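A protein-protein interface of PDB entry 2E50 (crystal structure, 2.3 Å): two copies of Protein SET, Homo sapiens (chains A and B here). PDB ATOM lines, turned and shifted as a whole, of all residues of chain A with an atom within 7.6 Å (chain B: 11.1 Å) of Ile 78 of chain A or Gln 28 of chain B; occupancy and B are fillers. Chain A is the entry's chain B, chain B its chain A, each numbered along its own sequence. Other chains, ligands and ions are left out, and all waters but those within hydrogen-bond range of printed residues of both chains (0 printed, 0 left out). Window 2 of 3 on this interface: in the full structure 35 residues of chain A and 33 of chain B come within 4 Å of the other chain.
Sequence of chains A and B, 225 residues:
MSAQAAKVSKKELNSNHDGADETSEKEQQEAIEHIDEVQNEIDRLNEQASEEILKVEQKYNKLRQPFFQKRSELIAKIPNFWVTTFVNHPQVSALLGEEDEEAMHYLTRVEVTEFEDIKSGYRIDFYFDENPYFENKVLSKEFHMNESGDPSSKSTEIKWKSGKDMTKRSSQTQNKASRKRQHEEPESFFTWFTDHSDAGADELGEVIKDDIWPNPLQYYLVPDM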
ATOM      1  N   SER A  72     -26.799  15.873  21.702  1.00  0.00           N
ATOM      2  CA  SER A  72     -26.585  17.312  21.975  1.00  0.00           C
ATOM      3  C   SER A  72     -25.861  17.647  23.255  1.00  0.00           C
ATOM      4  O   SER A  72     -24.922  18.441  23.199  1.00  0.00           O
ATOM      5  CB  SER A  72     -27.890  18.119  21.981  1.00  0.00           C
ATOM      6  OG  SER A  72     -28.394  18.046  20.659  1.00  0.00           O
ATOM      7  N   GLU A  73     -26.333  17.109  24.397  1.00  0.00           N
ATOM      8  CA  GLU A  73     -25.684  17.364  25.693  1.00  0.00           C
ATOM      9  C   GLU A  73     -24.219  16.892  25.705  1.00  0.00           C
ATOM     10  O   GLU A  73     -23.374  17.517  26.334  1.00  0.00           O
ATOM     11  CB  GLU A  73     -26.464  16.716  26.855  1.00  0.00           C
ATOM     12  CG  GLU A  73     -27.893  17.313  27.056  1.00  0.00           C
ATOM     13  CD  GLU A  73     -28.903  16.343  27.692  1.00  0.00           C
ATOM     14  OE1 GLU A  73     -28.492  15.234  28.145  1.00  0.00           O
ATOM     15  OE2 GLU A  73     -30.137  16.678  27.701  1.00  0.00           O
ATOM     16  N   LEU A  74     -23.922  15.790  25.016  1.00  0.00           N
ATOM     17  CA  LEU A  74     -22.571  15.218  25.004  1.00  0.00           C
ATOM     18  C   LEU A  74     -21.646  16.060  24.112  1.00  0.00           C
ATOM     19  O   LEU A  74     -20.545  16.331  24.495  1.00  0.00           O
ATOM     20  CB  LEU A  74     -22.598  13.747  24.538  1.00  0.00           C
ATOM     21  CG  LEU A  74     -23.374  12.797  25.442  1.00  0.00           C
ATOM     22  CD1 LEU A  74     -23.540  11.464  24.749  1.00  0.00           C
ATOM     23  CD2 LEU A  74     -22.646  12.648  26.850  1.00  0.00           C
ATOM     24  N   ILE A  75     -22.121  16.451  22.936  1.00  0.00           N
ATOM     25  CA  ILE A  75     -21.396  17.339  22.018  1.00  0.00           C
ATOM     26  C   ILE A  75     -21.021  18.678  22.642  1.00  0.00           C
ATOM     27  O   ILE A  75     -19.915  19.201  22.370  1.00  0.00           O
ATOM     28  CB  ILE A  75     -22.192  17.584  20.732  1.00  0.00           C
ATOM     29  CG1 ILE A  75     -22.228  16.305  19.873  1.00  0.00           C
ATOM     30  CG2 ILE A  75     -21.660  18.823  19.993  1.00  0.00           C
ATOM     31  CD1 ILE A  75     -23.307  16.277  18.767  1.00  0.00           C
ATOM     32  N   ALA A  76     -21.918  19.225  23.481  1.00  0.00           N
ATOM     33  CA  ALA A  76     -21.597  20.416  24.289  1.00  0.00           C
ATOM     34  C   ALA A  76     -20.273  20.323  25.093  1.00  0.00           C
ATOM     35  O   ALA A  76     -19.703  21.348  25.499  1.00  0.00           O
ATOM     36  CB  ALA A  76     -22.788  20.788  25.226  1.00  0.00           C
ATOM     37  N   LYS A  77     -19.795  19.104  25.333  1.00  0.00           N
ATOM     38  CA  LYS A  77     -18.592  18.875  26.134  1.00  0.00           C
ATOM     39  C   LYS A  77     -17.339  18.737  25.261  1.00  0.00           C
ATOM     40  O   LYS A  77     -16.245  18.495  25.774  1.00  0.00           O
ATOM     41  CB  LYS A  77     -18.744  17.617  26.976  1.00  0.00           C
ATOM     42  CG  LYS A  77     -19.981  17.595  27.819  1.00  0.00           C
ATOM     43  CD  LYS A  77     -19.883  16.540  28.876  1.00  0.00           C
ATOM     44  CE  LYS A  77     -20.660  16.926  30.158  1.00  0.00           C
ATOM     45  NZ  LYS A  77     -19.810  16.530  31.377  1.00  0.00           N
ATOM     46  N   ILE A  78     -17.519  18.843  23.941  1.00  0.00           N
ATOM     47  CA  ILE A  78     -16.418  18.841  22.983  1.00  0.00           C
ATOM     48  C   ILE A  78     -16.356  20.243  22.354  1.00  0.00           C
ATOM     49  O   ILE A  78     -17.194  20.587  21.518  1.00  0.00           O
ATOM     50  CB  ILE A  78     -16.540  17.769  21.877  1.00  0.00           C
ATOM     51  CG1 ILE A  78     -16.801  16.376  22.451  1.00  0.00           C
ATOM     52  CG2 ILE A  78     -15.280  17.761  21.015  1.00  0.00           C
ATOM     53  CD1 ILE A  78     -16.992  15.306  21.386  1.00  0.00           C
ATOM     54  N   PRO A  79     -15.350  21.060  22.774  1.00  0.00           N
ATOM     55  CA  PRO A  79     -15.296  22.406  22.218  1.00  0.00           C
ATOM     56  C   PRO A  79     -14.854  22.301  20.753  1.00  0.00           C
ATOM     57  O   PRO A  79     -14.023  21.431  20.427  1.00  0.00           O
ATOM     58  CB  PRO A  79     -14.244  23.116  23.077  1.00  0.00           C
ATOM     59  CG  PRO A  79     -13.884  22.144  24.219  1.00  0.00           C
ATOM     60  CD  PRO A  79     -14.244  20.783  23.706  1.00  0.00           C
ATOM     61  N   ASN A  80     -15.416  23.167  19.904  1.00  0.00           N
ATOM     62  CA  ASN A  80     -15.149  23.209  18.457  1.00  0.00           C
ATOM     63  C   ASN A  80     -15.646  21.969  17.689  1.00  0.00           C
ATOM     64  O   ASN A  80     -15.165  21.691  16.583  1.00  0.00           O
ATOM     65  CB  ASN A  80     -13.674  23.492  18.122  1.00  0.00           C
ATOM     66  CG  ASN A  80     -13.091  24.631  18.922  1.00  0.00           C
ATOM     67  OD1 ASN A  80     -13.595  25.764  18.901  1.00  0.00           O
ATOM     68  ND2 ASN A  80     -12.012  24.339  19.641  1.00  0.00           N
ATOM     69  N   PHE A  81     -16.639  21.261  18.248  1.00  0.00           N
ATOM     70  CA  PHE A  81     -17.145  20.060  17.621  1.00  0.00           C
ATOM     71  C   PHE A  81     -17.734  20.359  16.255  1.00  0.00           C
ATOM     72  O   PHE A  81     -17.428  19.651  15.307  1.00  0.00           O
ATOM     73  CB  PHE A  81     -18.133  19.277  18.520  1.00  0.00           C
ATOM     74  CG  PHE A  81     -18.724  18.041  17.841  1.00  0.00           C
ATOM     75  CD1 PHE A  81     -18.133  16.796  18.000  1.00  0.00           C
ATOM     76  CD2 PHE A  81     -19.857  18.134  17.016  1.00  0.00           C
ATOM     77  CE1 PHE A  81     -18.673  15.666  17.372  1.00  0.00           C
ATOM     78  CE2 PHE A  81     -20.378  16.996  16.358  1.00  0.00           C
ATOM     79  CZ  PHE A  81     -19.775  15.771  16.546  1.00  0.00           C
ATOM     80  N   TRP A  82     -18.570  21.405  16.143  1.00  0.00           N
ATOM     81  CA  TRP A  82     -19.316  21.642  14.894  1.00  0.00           C
ATOM     82  C   TRP A  82     -18.478  22.297  13.777  1.00  0.00           C
ATOM     83  O   TRP A  82     -18.644  21.981  12.582  1.00  0.00           O
ATOM     84  CB  TRP A  82     -20.668  22.362  15.173  1.00  0.00           C
ATOM     85  CG  TRP A  82     -21.703  21.376  15.684  1.00  0.00           C
ATOM     86  CD1 TRP A  82     -22.166  21.272  16.956  1.00  0.00           C
ATOM     87  CD2 TRP A  82     -22.323  20.310  14.944  1.00  0.00           C
ATOM     88  NE1 TRP A  82     -23.030  20.207  17.065  1.00  0.00           N
ATOM     89  CE2 TRP A  82     -23.159  19.611  15.841  1.00  0.00           C
ATOM     90  CE3 TRP A  82     -22.268  19.891  13.608  1.00  0.00           C
ATOM     91  CZ2 TRP A  82     -23.952  18.519  15.447  1.00  0.00           C
ATOM     92  CZ3 TRP A  82     -23.049  18.800  13.213  1.00  0.00           C
ATOM     93  CH2 TRP A  82     -23.884  18.128  14.136  1.00  0.00           C
ATOM     94  N   THR A  84     -15.131  21.781  13.472  1.00  0.00           N
ATOM     95  CA  THR A  84     -14.266  20.682  13.033  1.00  0.00           C
ATOM     96  C   THR A  84     -15.048  19.733  12.150  1.00  0.00           C
ATOM     97  O   THR A  84     -14.550  19.309  11.123  1.00  0.00           O
ATOM     98  CB  THR A  84     -13.718  19.916  14.236  1.00  0.00           C
ATOM     99  OG1 THR A  84     -13.145  20.849  15.139  1.00  0.00           O
ATOM    100  CG2 THR A  84     -12.667  18.872  13.842  1.00  0.00           C
ATOM    101  N   LEU A 107     -19.585  28.883  17.071  1.00  0.00           N
ATOM    102  CA  LEU A 107     -20.618  27.878  16.859  1.00  0.00           C
ATOM    103  C   LEU A 107     -20.613  26.829  17.964  1.00  0.00           C
ATOM    104  O   LEU A 107     -19.694  26.032  18.091  1.00  0.00           O
ATOM    105  CB  LEU A 107     -20.534  27.214  15.461  1.00  0.00           C
ATOM    106  CG  LEU A 107     -21.711  26.281  15.095  1.00  0.00           C
ATOM    107  CD1 LEU A 107     -23.040  27.013  15.045  1.00  0.00           C
ATOM    108  CD2 LEU A 107     -21.492  25.592  13.789  1.00  0.00           C
ATOM    109  N   THR A 108     -21.695  26.798  18.717  1.00  0.00           N
ATOM    110  CA  THR A 108     -21.767  25.998  19.916  1.00  0.00           C
ATOM    111  C   THR A 108     -22.578  24.678  19.744  1.00  0.00           C
ATOM    112  O   THR A 108     -22.358  23.673  20.447  1.00  0.00           O
ATOM    113  CB  THR A 108     -22.300  26.946  21.006  1.00  0.00           C
ATOM    114  OG1 THR A 108     -21.195  27.374  21.835  1.00  0.00           O
ATOM    115  CG2 THR A 108     -23.429  26.373  21.804  1.00  0.00           C
ATOM    116  N   LEU A 217     -19.981  12.396  14.010  1.00  0.00           N
ATOM    117  CA  LEU A 217     -18.692  11.826  14.401  1.00  0.00           C
ATOM    118  C   LEU A 217     -17.887  11.250  13.228  1.00  0.00           C
ATOM    119  O   LEU A 217     -16.630  11.202  13.241  1.00  0.00           O
ATOM    120  CB  LEU A 217     -18.895  10.721  15.461  1.00  0.00           C
ATOM    121  CG  LEU A 217     -18.836  10.962  16.992  1.00  0.00           C
ATOM    122  CD1 LEU A 217     -18.594   9.612  17.633  1.00  0.00           C
ATOM    123  CD2 LEU A 217     -17.723  11.927  17.462  1.00  0.00           C
ATOM    124  N   TYR A 220     -16.201  14.574  12.310  1.00  0.00           N
ATOM    125  CA  TYR A 220     -15.389  15.004  13.445  1.00  0.00           C
ATOM    126  C   TYR A 220     -14.063  14.248  13.613  1.00  0.00           C
ATOM    127  O   TYR A 220     -13.016  14.852  13.763  1.00  0.00           O
ATOM    128  CB  TYR A 220     -16.175  14.930  14.763  1.00  0.00           C
ATOM    129  CG  TYR A 220     -15.347  15.482  15.914  1.00  0.00           C
ATOM    130  CD1 TYR A 220     -14.752  14.644  16.831  1.00  0.00           C
ATOM    131  CD2 TYR A 220     -15.136  16.861  16.034  1.00  0.00           C
ATOM    132  CE1 TYR A 220     -13.963  15.168  17.875  1.00  0.00           C
ATOM    133  CE2 TYR A 220     -14.379  17.393  17.056  1.00  0.00           C
ATOM    134  CZ  TYR A 220     -13.801  16.550  17.974  1.00  0.00           C
ATOM    135  OH  TYR A 220     -13.063  17.099  18.980  1.00  0.00           O
ATOM    136  N   LEU A 221     -14.144  12.924  13.597  1.00  0.00           N
ATOM    137  CA  LEU A 221     -13.030  12.005  13.850  1.00  0.00           C
ATOM    138  C   LEU A 221     -12.113  11.661  12.658  1.00  0.00           C
ATOM    139  O   LEU A 221     -11.127  10.949  12.842  1.00  0.00           O
ATOM    140  CB  LEU A 221     -13.589  10.693  14.392  1.00  0.00           C
ATOM    141  CG  LEU A 221     -14.272  10.675  15.739  1.00  0.00           C
ATOM    142  CD1 LEU A 221     -14.800   9.302  15.967  1.00  0.00           C
ATOM    143  CD2 LEU A 221     -13.365  11.119  16.886  1.00  0.00           C
ATOM    144  N   ASP B  21      -5.059  19.524  30.469  1.00  0.00           N
ATOM    145  CA  ASP B  21      -4.826  18.288  29.728  1.00  0.00           C
ATOM    146  C   ASP B  21      -5.667  17.156  30.298  1.00  0.00           C
ATOM    147  O   ASP B  21      -6.722  16.836  29.754  1.00  0.00           O
ATOM    148  CB  ASP B  21      -3.331  17.920  29.732  1.00  0.00           C
ATOM    149  CG  ASP B  21      -2.485  18.886  28.901  1.00  0.00           C
ATOM    150  OD1 ASP B  21      -2.862  19.179  27.742  1.00  0.00           O
ATOM    151  OD2 ASP B  21      -1.434  19.347  29.405  1.00  0.00           O
ATOM    152  N   GLU B  22      -5.205  16.574  31.404  1.00  0.00           N
ATOM    153  CA  GLU B  22      -5.908  15.472  32.090  1.00  0.00           C
ATOM    154  C   GLU B  22      -7.304  15.886  32.620  1.00  0.00           C
ATOM    155  O   GLU B  22      -7.961  15.123  33.348  1.00  0.00           O
ATOM    156  CB  GLU B  22      -5.011  14.834  33.178  1.00  0.00           C
ATOM    157  CG  GLU B  22      -4.705  15.730  34.400  1.00  0.00           C
ATOM    158  CD  GLU B  22      -3.230  15.704  34.847  1.00  0.00           C
ATOM    159  OE1 GLU B  22      -2.541  14.665  34.680  1.00  0.00           O
ATOM    160  OE2 GLU B  22      -2.767  16.745  35.372  1.00  0.00           O
ATOM    161  N   THR B  23      -7.726  17.099  32.244  1.00  0.00           N
ATOM    162  CA  THR B  23      -9.115  17.566  32.380  1.00  0.00           C
ATOM    163  C   THR B  23      -9.813  17.635  31.009  1.00  0.00           C
ATOM    164  O   THR B  23     -10.771  16.898  30.775  1.00  0.00           O
ATOM    165  CB  THR B  23      -9.218  18.944  33.133  1.00  0.00           C
ATOM    166  OG1 THR B  23      -9.197  18.721  34.551  1.00  0.00           O
ATOM    167  CG2 THR B  23     -10.516  19.706  32.784  1.00  0.00           C
ATOM    168  N   SER B  24      -9.319  18.503  30.121  1.00  0.00           N
ATOM    169  CA  SER B  24      -9.986  18.810  28.852  1.00  0.00           C
ATOM    170  C   SER B  24      -9.913  17.653  27.838  1.00  0.00           C
ATOM    171  O   SER B  24     -10.925  17.290  27.221  1.00  0.00           O
ATOM    172  CB  SER B  24      -9.414  20.093  28.241  1.00  0.00           C
ATOM    173  OG  SER B  24     -10.301  20.660  27.286  1.00  0.00           O
ATOM    174  N   GLU B  25      -8.714  17.087  27.679  1.00  0.00           N
ATOM    175  CA  GLU B  25      -8.494  15.952  26.792  1.00  0.00           C
ATOM    176  C   GLU B  25      -9.350  14.745  27.180  1.00  0.00           C
ATOM    177  O   GLU B  25     -10.111  14.223  26.349  1.00  0.00           O
ATOM    178  CB  GLU B  25      -7.006  15.577  26.741  1.00  0.00           C
ATOM    179  CG  GLU B  25      -6.706  14.362  25.896  1.00  0.00           C
ATOM    180  CD  GLU B  25      -7.290  14.458  24.487  1.00  0.00           C
ATOM    181  OE1 GLU B  25      -7.425  13.412  23.817  1.00  0.00           O
ATOM    182  OE2 GLU B  25      -7.624  15.579  24.044  1.00  0.00           O
ATOM    183  N   LYS B  26      -9.214  14.319  28.433  1.00  0.00           N
ATOM    184  CA  LYS B  26     -10.051  13.267  29.009  1.00  0.00           C
ATOM    185  C   LYS B  26     -11.559  13.550  28.835  1.00  0.00           C
ATOM    186  O   LYS B  26     -12.331  12.645  28.506  1.00  0.00           O
ATOM    187  CB  LYS B  26      -9.699  13.060  30.496  1.00  0.00           C
ATOM    188  CG  LYS B  26     -10.407  11.881  31.210  1.00  0.00           C
ATOM    189  CD  LYS B  26      -9.919  10.496  30.699  1.00  0.00           C
ATOM    190  CE  LYS B  26     -10.377   9.354  31.628  1.00  0.00           C
ATOM    191  NZ  LYS B  26     -10.128   7.993  31.057  1.00  0.00           N
ATOM    192  N   GLU B  27     -11.970  14.800  29.028  1.00  0.00           N
ATOM    193  CA  GLU B  27     -13.382  15.147  28.943  1.00  0.00           C
ATOM    194  C   GLU B  27     -13.882  14.839  27.541  1.00  0.00           C
ATOM    195  O   GLU B  27     -14.894  14.168  27.363  1.00  0.00           O
ATOM    196  CB  GLU B  27     -13.612  16.630  29.250  1.00  0.00           C
ATOM    197  CG  GLU B  27     -14.610  16.899  30.383  1.00  0.00           C
ATOM    198  CD  GLU B  27     -13.933  16.998  31.757  1.00  0.00           C
ATOM    199  OE1 GLU B  27     -13.240  16.043  32.180  1.00  0.00           O
ATOM    200  OE2 GLU B  27     -14.100  18.042  32.422  1.00  0.00           O
ATOM    201  N   GLN B  28     -13.141  15.361  26.571  1.00  0.00           N
ATOM    202  CA  GLN B  28     -13.338  15.163  25.152  1.00  0.00           C
ATOM    203  C   GLN B  28     -13.417  13.652  24.776  1.00  0.00           C
ATOM    204  O   GLN B  28     -14.366  13.212  24.130  1.00  0.00           O
ATOM    205  CB  GLN B  28     -12.165  15.848  24.427  1.00  0.00           C
ATOM    206  CG  GLN B  28     -12.467  16.319  23.010  1.00  0.00           C
ATOM    207  CD  GLN B  28     -11.398  15.949  21.992  1.00  0.00           C
ATOM    208  OE1 GLN B  28     -10.201  15.976  22.275  1.00  0.00           O
ATOM    209  NE2 GLN B  28     -11.833  15.623  20.795  1.00  0.00           N
ATOM    210  N   GLN B  29     -12.436  12.877  25.230  1.00  0.00           N
ATOM    211  CA  GLN B  29     -12.307  11.469  24.900  1.00  0.00           C
ATOM    212  C   GLN B  29     -13.425  10.660  25.486  1.00  0.00           C
ATOM    213  O   GLN B  29     -13.837   9.640  24.930  1.00  0.00           O
ATOM    214  CB  GLN B  29     -10.987  10.916  25.414  1.00  0.00           C
ATOM    215  CG  GLN B  29      -9.860  11.132  24.468  1.00  0.00           C
ATOM    216  CD  GLN B  29      -8.541  10.721  25.038  1.00  0.00           C
ATOM    217  OE1 GLN B  29      -8.458   9.868  25.906  1.00  0.00           O
ATOM    218  NE2 GLN B  29      -7.494  11.306  24.528  1.00  0.00           N
ATOM    219  N   GLU B  30     -13.907  11.119  26.614  1.00  0.00           N
ATOM    220  CA  GLU B  30     -14.991  10.457  27.293  1.00  0.00           C
ATOM    221  C   GLU B  30     -16.303  10.749  26.584  1.00  0.00           C
ATOM    222  O   GLU B  30     -17.091   9.842  26.364  1.00  0.00           O
ATOM    223  CB  GLU B  30     -15.080  10.982  28.722  1.00  0.00           C
ATOM    224  CG  GLU B  30     -13.970  10.499  29.568  1.00  0.00           C
ATOM    225  CD  GLU B  30     -14.364   9.260  30.293  1.00  0.00           C
ATOM    226  OE1 GLU B  30     -14.040   9.175  31.513  1.00  0.00           O
ATOM    227  OE2 GLU B  30     -15.022   8.400  29.642  1.00  0.00           O
ATOM    228  N   ALA B  31     -16.501  12.025  26.244  1.00  0.00           N
ATOM    229  CA  ALA B  31     -17.664  12.466  25.507  1.00  0.00           C
ATOM    230  C   ALA B  31     -17.791  11.720  24.191  1.00  0.00           C
ATOM    231  O   ALA B  31     -18.891  11.354  23.813  1.00  0.00           O
ATOM    232  CB  ALA B  31     -17.626  13.974  25.266  1.00  0.00           C
ATOM    233  N   ILE B  32     -16.669  11.487  23.513  1.00  0.00           N
ATOM    234  CA  ILE B  32     -16.671  10.848  22.196  1.00  0.00           C
ATOM    235  C   ILE B  32     -17.160   9.416  22.320  1.00  0.00           C
ATOM    236  O   ILE B  32     -17.937   8.934  21.480  1.00  0.00           O
ATOM    237  CB  ILE B  32     -15.246  10.863  21.598  1.00  0.00           C
ATOM    238  CG1 ILE B  32     -14.906  12.238  21.029  1.00  0.00           C
ATOM    239  CG2 ILE B  32     -15.035   9.751  20.555  1.00  0.00           C
ATOM    240  CD1 ILE B  32     -13.401  12.361  20.608  1.00  0.00           C
ATOM    241  N   GLU B  33     -16.680   8.737  23.360  1.00  0.00           N
ATOM    242  CA  GLU B  33     -17.078   7.381  23.638  1.00  0.00           C
ATOM    243  C   GLU B  33     -18.567   7.294  24.004  1.00  0.00           C
ATOM    244  O   GLU B  33     -19.241   6.344  23.604  1.00  0.00           O
ATOM    245  CB  GLU B  33     -16.228   6.780  24.760  1.00  0.00           C
ATOM    246  CG  GLU B  33     -16.661   5.383  25.151  1.00  0.00           C
ATOM    247  CD  GLU B  33     -15.719   4.749  26.148  1.00  0.00           C
ATOM    248  OE1 GLU B  33     -15.964   3.618  26.585  1.00  0.00           O
ATOM    249  OE2 GLU B  33     -14.696   5.362  26.488  1.00  0.00           O
ATOM    250  N   HIS B  34     -19.064   8.282  24.749  1.00  0.00           N
ATOM    251  CA  HIS B  34     -20.460   8.343  25.105  1.00  0.00           C
ATOM    252  C   HIS B  34     -21.337   8.714  23.910  1.00  0.00           C
ATOM    253  O   HIS B  34     -22.463   8.246  23.821  1.00  0.00           O
ATOM    254  CB  HIS B  34     -20.702   9.351  26.253  1.00  0.00           C
ATOM    255  CG  HIS B  34     -20.008   9.006  27.527  1.00  0.00           C
ATOM    256  ND1 HIS B  34     -19.636   9.958  28.457  1.00  0.00           N
ATOM    257  CD2 HIS B  34     -19.624   7.810  28.034  1.00  0.00           C
ATOM    258  CE1 HIS B  34     -19.033   9.361  29.471  1.00  0.00           C
ATOM    259  NE2 HIS B  34     -19.014   8.058  29.237  1.00  0.00           N
ATOM    260  N   ILE B  35     -20.847   9.558  23.008  1.00  0.00           N
ATOM    261  CA  ILE B  35     -21.587   9.850  21.778  1.00  0.00           C
ATOM    262  C   ILE B  35     -21.717   8.600  20.899  1.00  0.00           C
ATOM    263  O   ILE B  35     -22.749   8.365  20.310  1.00  0.00           O
ATOM    264  CB  ILE B  35     -20.956  11.009  20.969  1.00  0.00           C
ATOM    265  CG1 ILE B  35     -21.151  12.324  21.727  1.00  0.00           C
ATOM    266  CG2 ILE B  35     -21.544  11.084  19.479  1.00  0.00           C
ATOM    267  CD1 ILE B  35     -20.154  13.381  21.391  1.00  0.00           C
ATOM    268  N   ASP B  36     -20.658   7.810  20.825  1.00  0.00           N
ATOM    269  CA  ASP B  36     -20.674   6.610  20.035  1.00  0.00           C
ATOM    270  C   ASP B  36     -21.746   5.664  20.559  1.00  0.00           C
ATOM    271  O   ASP B  36     -22.428   5.025  19.766  1.00  0.00           O
ATOM    272  CB  ASP B  36     -19.295   5.913  20.047  1.00  0.00           C
ATOM    273  CG  ASP B  36     -19.313   4.609  19.285  1.00  0.00           C
ATOM    274  OD1 ASP B  36     -19.186   3.545  19.914  1.00  0.00           O
ATOM    275  OD2 ASP B  36     -19.511   4.625  18.052  1.00  0.00           O
ATOM    276  N   GLU B  37     -21.856   5.553  21.883  1.00  0.00           N
ATOM    277  CA  GLU B  37     -22.871   4.710  22.511  1.00  0.00           C
ATOM    278  C   GLU B  37     -24.283   5.122  22.065  1.00  0.00           C
ATOM    279  O   GLU B  37     -25.083   4.299  21.653  1.00  0.00           O
ATOM    280  CB  GLU B  37     -22.721   4.712  24.034  1.00  0.00           C
ATOM    281  CG  GLU B  37     -21.391   4.032  24.511  1.00  0.00           C
ATOM    282  CD  GLU B  37     -21.092   4.252  25.992  1.00  0.00           C
ATOM    283  OE1 GLU B  37     -21.897   4.915  26.699  1.00  0.00           O
ATOM    284  OE2 GLU B  37     -20.052   3.757  26.461  1.00  0.00           O
ATOM    285  N   GLN B  39     -25.001   7.023  19.361  1.00  0.00           N
ATOM    286  CA  GLN B  39     -25.058   6.665  17.922  1.00  0.00           C
ATOM    287  C   GLN B  39     -25.490   5.261  17.612  1.00  0.00           C
ATOM    288  O   GLN B  39     -26.136   5.026  16.564  1.00  0.00           O
ATOM    289  CB  GLN B  39     -23.709   6.829  17.170  1.00  0.00           C
ATOM    290  CG  GLN B  39     -23.425   8.219  16.602  1.00  0.00           C
ATOM    291  CD  GLN B  39     -24.593   8.933  15.917  1.00  0.00           C
ATOM    292  OE1 GLN B  39     -24.839  10.101  16.224  1.00  0.00           O
ATOM    293  NE2 GLN B  39     -25.313   8.262  14.984  1.00  0.00           N
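NE2 of Gln 28 of chain B lies within hydrogen-bond range of OH of Tyr 220 of chain A (2.6 Å).
The side-chain amide oxygen (OE1) of Gln 28 of chain B sits close to the side-chain carboxylate (OE2) of Glu 25 of chain B (3.2 Å). A ring nitrogen (ND1) of His 34 of chain B lies close to the backbone carbonyl oxygen (O) of Glu 30 of chain B.
Leu 74 of chain A touches Ala 31 of chain B (O to CB, 3.8 Å). Ile 35 of chain B touches Leu 74 of chain A. Ile 75 of chain A touches Ile 35 of chain B. CG2 of Ile 78 of chain A touches CG of Gln 28 of chain B, 3.7 Å away. Ala 31 of chain B touches Ile 78 of chain A. CD1 of Ile 78 of chain A touches CG1 of Ile 32 of chain B, 3.7 Å away. Ile 78 of chain A touches Ile 35 of chain B (CD1 to CD1, 3.7 Å). Leu 217 of chain A touches Ile 32 of chain B. Leu 217 of chain A touches Ile 35 of chain B (CG to CG2, 3.7 Å). Leu 221 of chain A touches Ile 32 of chain B.
No residue of chain B comes within 4 Å of Ala 76 of chain A. Lys 77 of chain A touches none of the printed residues of chain B. Of the printed residues of chain B, Ile 78 of chain A touches Gln 28, Ala 31, Ile 32 and Ile 35. No residue of chain B comes within 4 Å of Asn 80 of chain A. No residue of chain B comes within 4 Å of Phe 81 of chain A. Of chain A, only Ile 78 (3.7 Å) and Tyr 220 (2.6 Å) come within 4 Å of Gln 28 of chain B. Printed residues of chain A within 4 Å of Ile 32 of chain B: Ile 78 (3.7 Å), Leu 217 (3.96 Å), Tyr 220 (3.96 Å) and Leu 221 (3.9 Å). Of the printed residues of chain A, His 34 of chain B touches Leu 74 (3.5 Å). Printed residues of chain A within 4 Å of Ile 35 of chain B: Leu 74 (3.5 Å), Ile 75 (3.9 Å), Ile 78 (3.7 Å) and Leu 217 (3.7 Å). Gln 39 of chain B touches none of the printed residues of chain A.
Hydrophobic or aromatic side chains of chain B within 4 Å of the printed part of chain A: Ala 31, Ile 32, His 34 and Ile 35. Of the 17 printed residues of chain A, 6 touch a printed residue of chain B. Printed residues of chain A that touch a printed residue of chain B: Leu 74, Ile 75, Ile 78, Leu 217, Tyr 220 and Leu 221. Hydrophobic or aromatic side chains of chain A that line the printed part of chain B: Leu 74, Ile 75, Ile 78, Leu 217, Tyr 220 and Leu 221. Along chain A the printed residues that touch a printed residue of chain B span positions 74 to 221. Among the printed residues, 13 pairs touch across the chains. Among the printed residues, no Asp or Glu carboxylate lies within 4 Å of a Lys or Arg side-chain nitrogen of the other chain.
No position is printed for both chains. Of the 13 pairs that touch across the chains among the printed residues, none has its exchanged pair printed and touching as well.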
